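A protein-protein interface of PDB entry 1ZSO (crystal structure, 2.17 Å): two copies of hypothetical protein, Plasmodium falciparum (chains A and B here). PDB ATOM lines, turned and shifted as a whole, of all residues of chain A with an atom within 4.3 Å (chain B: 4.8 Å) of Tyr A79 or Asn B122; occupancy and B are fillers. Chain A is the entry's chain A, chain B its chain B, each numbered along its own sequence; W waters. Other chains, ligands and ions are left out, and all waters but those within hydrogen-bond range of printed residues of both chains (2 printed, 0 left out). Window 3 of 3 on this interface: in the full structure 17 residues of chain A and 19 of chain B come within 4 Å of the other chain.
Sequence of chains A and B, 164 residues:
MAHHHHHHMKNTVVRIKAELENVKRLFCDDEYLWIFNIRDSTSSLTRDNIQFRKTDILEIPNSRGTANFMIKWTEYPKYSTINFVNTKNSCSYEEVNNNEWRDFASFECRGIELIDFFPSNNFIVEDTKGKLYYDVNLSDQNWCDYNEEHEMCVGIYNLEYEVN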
ATOM      1  N   PRO A  61       8.104 -25.623  -5.324  1.00  0.00           N
ATOM      2  CA  PRO A  61       9.178 -25.157  -4.476  1.00  0.00           C
ATOM      3  C   PRO A  61       8.599 -24.442  -3.289  1.00  0.00           C
ATOM      4  O   PRO A  61       7.533 -23.837  -3.411  1.00  0.00           O
ATOM      5  CB  PRO A  61       9.910 -24.159  -5.366  1.00  0.00           C
ATOM      6  CG  PRO A  61       9.612 -24.620  -6.725  1.00  0.00           C
ATOM      7  CD  PRO A  61       8.195 -25.035  -6.663  1.00  0.00           C
ATOM      8  N   MET A  70       2.389 -25.880 -13.698  1.00  0.00           N
ATOM      9  CA  MET A  70       3.129 -24.694 -13.334  1.00  0.00           C
ATOM     10  C   MET A  70       3.928 -24.025 -14.405  1.00  0.00           C
ATOM     11  O   MET A  70       4.283 -24.597 -15.424  1.00  0.00           O
ATOM     12  CB  MET A  70       4.030 -24.892 -12.119  1.00  0.00           C
ATOM     13  CG  MET A  70       4.657 -26.190 -11.851  1.00  0.00           C
ATOM     14  SD  MET A  70       5.532 -25.968  -9.987  1.00  0.00           S
ATOM     15  CE  MET A  70       5.346 -24.210  -9.746  1.00  0.00           C
ATOM     16  N   ILE A  71       4.254 -22.784 -14.124  1.00  0.00           N
ATOM     17  CA  ILE A  71       5.030 -22.012 -15.039  1.00  0.00           C
ATOM     18  C   ILE A  71       5.831 -21.005 -14.247  1.00  0.00           C
ATOM     19  O   ILE A  71       5.374 -20.515 -13.239  1.00  0.00           O
ATOM     20  CB  ILE A  71       4.103 -21.364 -16.114  1.00  0.00           C
ATOM     21  CG1 ILE A  71       4.954 -20.725 -17.212  1.00  0.00           C
ATOM     22  CG2 ILE A  71       3.142 -20.365 -15.486  1.00  0.00           C
ATOM     23  CD1 ILE A  71       4.153 -20.055 -18.300  1.00  0.00           C
ATOM     24  N   LYS A  72       7.063 -20.803 -14.682  1.00  0.00           N
ATOM     25  CA  LYS A  72       7.923 -19.716 -14.285  1.00  0.00           C
ATOM     26  C   LYS A  72       7.841 -18.638 -15.363  1.00  0.00           C
ATOM     27  O   LYS A  72       8.404 -18.792 -16.442  1.00  0.00           O
ATOM     28  CB  LYS A  72       9.352 -20.230 -14.214  1.00  0.00           C
ATOM     29  CG  LYS A  72      10.302 -19.242 -13.580  1.00  0.00           C
ATOM     30  CD  LYS A  72      11.360 -19.909 -12.767  1.00  0.00           C
ATOM     31  CE  LYS A  72      12.768 -19.448 -13.178  1.00  0.00           C
ATOM     32  NZ  LYS A  72      12.948 -18.000 -13.037  1.00  0.00           N
ATOM     33  N   LYS A  78      10.290 -17.586  -9.132  1.00  0.00           N
ATOM     34  CA  LYS A  78       8.928 -17.626  -8.633  1.00  0.00           C
ATOM     35  C   LYS A  78       8.059 -18.382  -9.620  1.00  0.00           C
ATOM     36  O   LYS A  78       8.083 -18.090 -10.814  1.00  0.00           O
ATOM     37  CB  LYS A  78       8.418 -16.206  -8.466  1.00  0.00           C
ATOM     38  CG  LYS A  78       6.952 -16.061  -8.147  1.00  0.00           C
ATOM     39  CD  LYS A  78       6.627 -14.582  -8.180  1.00  0.00           C
ATOM     40  CE  LYS A  78       5.149 -14.251  -7.871  1.00  0.00           C
ATOM     41  NZ  LYS A  78       4.979 -12.744  -7.865  1.00  0.00           N
ATOM     42  N   TYR A  79       7.324 -19.369  -9.105  1.00  0.00           N
ATOM     43  CA  TYR A  79       6.527 -20.290  -9.913  1.00  0.00           C
ATOM     44  C   TYR A  79       5.052 -20.022  -9.670  1.00  0.00           C
ATOM     45  O   TYR A  79       4.623 -19.743  -8.559  1.00  0.00           O
ATOM     46  CB  TYR A  79       6.879 -21.760  -9.572  1.00  0.00           C
ATOM     47  CG  TYR A  79       8.264 -22.183 -10.048  1.00  0.00           C
ATOM     48  CD1 TYR A  79       9.401 -21.697  -9.431  1.00  0.00           C
ATOM     49  CD2 TYR A  79       8.423 -23.032 -11.156  1.00  0.00           C
ATOM     50  CE1 TYR A  79      10.701 -22.039  -9.901  1.00  0.00           C
ATOM     51  CE2 TYR A  79       9.671 -23.397 -11.617  1.00  0.00           C
ATOM     52  CZ  TYR A  79      10.823 -22.887 -10.998  1.00  0.00           C
ATOM     53  OH  TYR A  79      12.096 -23.244 -11.444  1.00  0.00           O
ATOM     54  N   SER A  80       4.285 -20.084 -10.731  1.00  0.00           N
ATOM     55  CA  SER A  80       2.858 -19.872 -10.670  1.00  0.00           C
ATOM     56  C   SER A  80       2.186 -21.212 -10.992  1.00  0.00           C
ATOM     57  O   SER A  80       2.778 -22.099 -11.660  1.00  0.00           O
ATOM     58  CB  SER A  80       2.492 -18.815 -11.697  1.00  0.00           C
ATOM     59  OG  SER A  80       3.323 -17.675 -11.512  1.00  0.00           O
ATOM     60  N   CYS B  28      23.569 -29.774 -11.664  1.00  0.00           N
ATOM     61  CA  CYS B  28      22.246 -29.371 -11.218  1.00  0.00           C
ATOM     62  C   CYS B  28      21.516 -30.469 -10.442  1.00  0.00           C
ATOM     63  O   CYS B  28      21.944 -31.619 -10.426  1.00  0.00           O
ATOM     64  CB  CYS B  28      21.437 -28.909 -12.401  1.00  0.00           C
ATOM     65  SG  CYS B  28      21.473 -30.023 -13.793  1.00  0.00           S
ATOM     66  N   ASP B  29      20.432 -30.100  -9.766  1.00  0.00           N
ATOM     67  CA  ASP B  29      19.713 -31.035  -8.912  1.00  0.00           C
ATOM     68  C   ASP B  29      18.338 -31.369  -9.504  1.00  0.00           C
ATOM     69  O   ASP B  29      18.087 -31.121 -10.672  1.00  0.00           O
ATOM     70  CB  ASP B  29      19.591 -30.447  -7.498  1.00  0.00           C
ATOM     71  CG  ASP B  29      18.578 -29.289  -7.413  1.00  0.00           C
ATOM     72  OD1 ASP B  29      17.935 -29.143  -6.342  1.00  0.00           O
ATOM     73  OD2 ASP B  29      18.405 -28.533  -8.407  1.00  0.00           O
ATOM     74  N   GLU B  31      15.517 -30.005  -8.760  1.00  0.00           N
ATOM     75  CA  GLU B  31      14.813 -28.746  -8.980  1.00  0.00           C
ATOM     76  C   GLU B  31      15.136 -28.145 -10.364  1.00  0.00           C
ATOM     77  O   GLU B  31      14.437 -27.268 -10.833  1.00  0.00           O
ATOM     78  CB  GLU B  31      15.168 -27.715  -7.874  1.00  0.00           C
ATOM     79  CG  GLU B  31      14.990 -28.194  -6.414  1.00  0.00           C
ATOM     80  CD  GLU B  31      15.558 -27.193  -5.352  1.00  0.00           C
ATOM     81  OE1 GLU B  31      15.458 -25.952  -5.564  1.00  0.00           O
ATOM     82  OE2 GLU B  31      16.088 -27.646  -4.291  1.00  0.00           O
ATOM     83  N   TYR B  32      16.189 -28.611 -11.026  1.00  0.00           N
ATOM     84  CA  TYR B  32      16.614 -27.967 -12.230  1.00  0.00           C
ATOM     85  C   TYR B  32      15.443 -27.831 -13.223  1.00  0.00           C
ATOM     86  O   TYR B  32      14.666 -28.784 -13.495  1.00  0.00           O
ATOM     87  CB  TYR B  32      17.824 -28.684 -12.882  1.00  0.00           C
ATOM     88  CG  TYR B  32      18.321 -27.925 -14.082  1.00  0.00           C
ATOM     89  CD1 TYR B  32      19.119 -26.819 -13.936  1.00  0.00           C
ATOM     90  CD2 TYR B  32      17.879 -28.245 -15.362  1.00  0.00           C
ATOM     91  CE1 TYR B  32      19.524 -26.080 -15.050  1.00  0.00           C
ATOM     92  CE2 TYR B  32      18.259 -27.522 -16.451  1.00  0.00           C
ATOM     93  CZ  TYR B  32      19.108 -26.438 -16.296  1.00  0.00           C
ATOM     94  OH  TYR B  32      19.476 -25.694 -17.401  1.00  0.00           O
ATOM     95  N   LEU B  33      15.330 -26.623 -13.769  1.00  0.00           N
ATOM     96  CA  LEU B  33      14.273 -26.313 -14.730  1.00  0.00           C
ATOM     97  C   LEU B  33      14.718 -26.531 -16.159  1.00  0.00           C
ATOM     98  O   LEU B  33      15.455 -25.690 -16.704  1.00  0.00           O
ATOM     99  CB  LEU B  33      13.794 -24.873 -14.578  1.00  0.00           C
ATOM    100  CG  LEU B  33      12.510 -24.692 -15.362  1.00  0.00           C
ATOM    101  CD1 LEU B  33      11.479 -25.641 -14.789  1.00  0.00           C
ATOM    102  CD2 LEU B  33      12.004 -23.265 -15.301  1.00  0.00           C
ATOM    103  N   ARG B  53      10.621 -30.347 -14.966  1.00  0.00           N
ATOM    104  CA  ARG B  53      11.643 -30.962 -14.084  1.00  0.00           C
ATOM    105  C   ARG B  53      11.635 -32.479 -14.179  1.00  0.00           C
ATOM    106  O   ARG B  53      10.592 -33.073 -14.416  1.00  0.00           O
ATOM    107  CB  ARG B  53      11.384 -30.600 -12.630  1.00  0.00           C
ATOM    108  CG  ARG B  53      11.658 -29.134 -12.309  1.00  0.00           C
ATOM    109  CD  ARG B  53      10.550 -28.567 -11.454  1.00  0.00           C
ATOM    110  NE  ARG B  53       9.250 -28.781 -12.121  1.00  0.00           N
ATOM    111  CZ  ARG B  53       8.703 -27.939 -13.003  1.00  0.00           C
ATOM    112  NH1 ARG B  53       9.319 -26.794 -13.296  1.00  0.00           N
ATOM    113  NH2 ARG B  53       7.536 -28.241 -13.582  1.00  0.00           N
ATOM    114  N   SER B 120      19.175 -22.605 -17.642  1.00  0.00           N
ATOM    115  CA  SER B 120      18.364 -21.808 -16.761  1.00  0.00           C
ATOM    116  C   SER B 120      19.291 -21.230 -15.709  1.00  0.00           C
ATOM    117  O   SER B 120      20.487 -21.119 -15.933  1.00  0.00           O
ATOM    118  CB  SER B 120      17.214 -22.646 -16.175  1.00  0.00           C
ATOM    119  OG  SER B 120      17.704 -23.704 -15.360  1.00  0.00           O
ATOM    120  N   ASN B 121      18.747 -20.831 -14.573  1.00  0.00           N
ATOM    121  CA  ASN B 121      19.590 -20.296 -13.508  1.00  0.00           C
ATOM    122  C   ASN B 121      19.422 -21.039 -12.208  1.00  0.00           C
ATOM    123  O   ASN B 121      19.396 -20.437 -11.153  1.00  0.00           O
ATOM    124  CB  ASN B 121      19.370 -18.783 -13.339  1.00  0.00           C
ATOM    125  CG  ASN B 121      18.037 -18.333 -13.867  1.00  0.00           C
ATOM    126  OD1 ASN B 121      17.955 -17.738 -14.958  1.00  0.00           O
ATOM    127  ND2 ASN B 121      16.968 -18.633 -13.119  1.00  0.00           N
ATOM    128  N   ASN B 122      19.283 -22.355 -12.289  1.00  0.00           N
ATOM    129  CA  ASN B 122      19.346 -23.159 -11.083  1.00  0.00           C
ATOM    130  C   ASN B 122      20.543 -24.105 -11.137  1.00  0.00           C
ATOM    131  O   ASN B 122      20.468 -25.224 -10.646  1.00  0.00           O
ATOM    132  CB  ASN B 122      18.066 -24.011 -10.738  1.00  0.00           C
ATOM    133  CG  ASN B 122      16.812 -23.668 -11.545  1.00  0.00           C
ATOM    134  OD1 ASN B 122      16.738 -23.853 -12.766  1.00  0.00           O
ATOM    135  ND2 ASN B 122      15.771 -23.301 -10.826  1.00  0.00           N
ATOM    136  N   PHE B 123      21.660 -23.679 -11.695  1.00  0.00           N
ATOM    137  CA  PHE B 123      22.849 -24.541 -11.631  1.00  0.00           C
ATOM    138  C   PHE B 123      23.499 -24.379 -10.278  1.00  0.00           C
ATOM    139  O   PHE B 123      23.212 -23.447  -9.555  1.00  0.00           O
ATOM    140  CB  PHE B 123      23.859 -24.227 -12.727  1.00  0.00           C
ATOM    141  CG  PHE B 123      23.409 -24.621 -14.090  1.00  0.00           C
ATOM    142  CD1 PHE B 123      23.577 -25.914 -14.530  1.00  0.00           C
ATOM    143  CD2 PHE B 123      22.809 -23.697 -14.940  1.00  0.00           C
ATOM    144  CE1 PHE B 123      23.161 -26.296 -15.781  1.00  0.00           C
ATOM    145  CE2 PHE B 123      22.408 -24.059 -16.196  1.00  0.00           C
ATOM    146  CZ  PHE B 123      22.597 -25.374 -16.627  1.00  0.00           C
ATOM    147  N   ILE B 124      24.343 -25.340  -9.938  1.00  0.00           N
ATOM    148  CA  ILE B 124      25.071 -25.373  -8.695  1.00  0.00           C
ATOM    149  C   ILE B 124      26.525 -25.508  -9.132  1.00  0.00           C
ATOM    150  O   ILE B 124      26.842 -26.217 -10.096  1.00  0.00           O
ATOM    151  CB  ILE B 124      24.636 -26.545  -7.775  1.00  0.00           C
ATOM    152  CG1 ILE B 124      23.104 -26.551  -7.625  1.00  0.00           C
ATOM    153  CG2 ILE B 124      25.336 -26.469  -6.367  1.00  0.00           C
ATOM    154  CD1 ILE B 124      22.540 -27.722  -6.816  1.00  0.00           C
ATOM    155  N   ASP B 135      21.902 -20.998  -7.388  1.00  0.00           N
ATOM    156  CA  ASP B 135      21.235 -20.066  -8.275  1.00  0.00           C
ATOM    157  C   ASP B 135      22.261 -19.529  -9.277  1.00  0.00           C
ATOM    158  O   ASP B 135      22.281 -18.341  -9.582  1.00  0.00           O
ATOM    159  CB  ASP B 135      20.641 -18.921  -7.448  1.00  0.00           C
ATOM    160  CG  ASP B 135      19.450 -19.367  -6.583  1.00  0.00           C
ATOM    161  OD1 ASP B 135      18.399 -19.733  -7.174  1.00  0.00           O
ATOM    162  OD2 ASP B 135      19.558 -19.326  -5.323  1.00  0.00           O
ATOM    163  N   VAL B 136      23.133 -20.412  -9.747  1.00  0.00           N
ATOM    164  CA  VAL B 136      24.148 -20.052 -10.740  1.00  0.00           C
ATOM    165  C   VAL B 136      23.449 -19.871 -12.073  1.00  0.00           C
ATOM    166  O   VAL B 136      22.765 -20.770 -12.568  1.00  0.00           O
ATOM    167  CB  VAL B 136      25.268 -21.103 -10.820  1.00  0.00           C
ATOM    168  CG1 VAL B 136      26.185 -20.847 -11.990  1.00  0.00           C
ATOM    169  CG2 VAL B 136      26.061 -21.129  -9.506  1.00  0.00           C
HETATM  170  O   HOH W   1       6.147 -27.103 -15.935  1.00  0.00           O
HETATM  171  O   HOH W   2       7.431 -24.628 -14.699  1.00  0.00           O
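The side-chain hydroxyl (OG) of Ser B120 lies within hydrogen-bond range of the side-chain amide oxygen (OD1) of Asn B122 (2.8 Å). The backbone NH of Leu B33 lies within hydrogen-bond range of the side-chain amide oxygen of Asn B122 (3.3 Å). O of Leu B33 is in hydrogen-bond range of OG of Ser B120, at 3.3 Å.
Among the printed residues, pairs that only touch across the chains: Tyr A79 with Asn B122 (3.7 Å), Tyr A79 with Arg B53 (3.8 Å), Tyr A79 with Leu B33 (3.9 Å) and Met A70 with Arg B53 (3.9 Å).
Asn B122 touches just one residue of chain A: Tyr A79. Printed residues of chain A within 4 Å of Arg B53: Met A70 and Tyr A79. Of the printed residues of chain A, Leu B33 touches Tyr A79. Printed residues of chain B within 4 Å of Met A70: Arg B53. The nearest residue of chain B that does not touch Tyr A79 is Glu B31 (4.7 Å). The nearest printed residue of chain A that does not touch Asn B122 is Lys A72 (5.4 Å).
Along chain B the printed residues that touch a printed residue of chain A span positions 33 to 122.
No position is printed for both chains.
Water W1 lies within hydrogen-bond range of the guanidinium group (NH2) of Arg B53 (3.0 Å) and the backbone carbonyl oxygen (O) of Met A70 (3.2 Å). Water W2 lies within hydrogen-bond range of NH1 of Arg B53 and O of Met A70.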
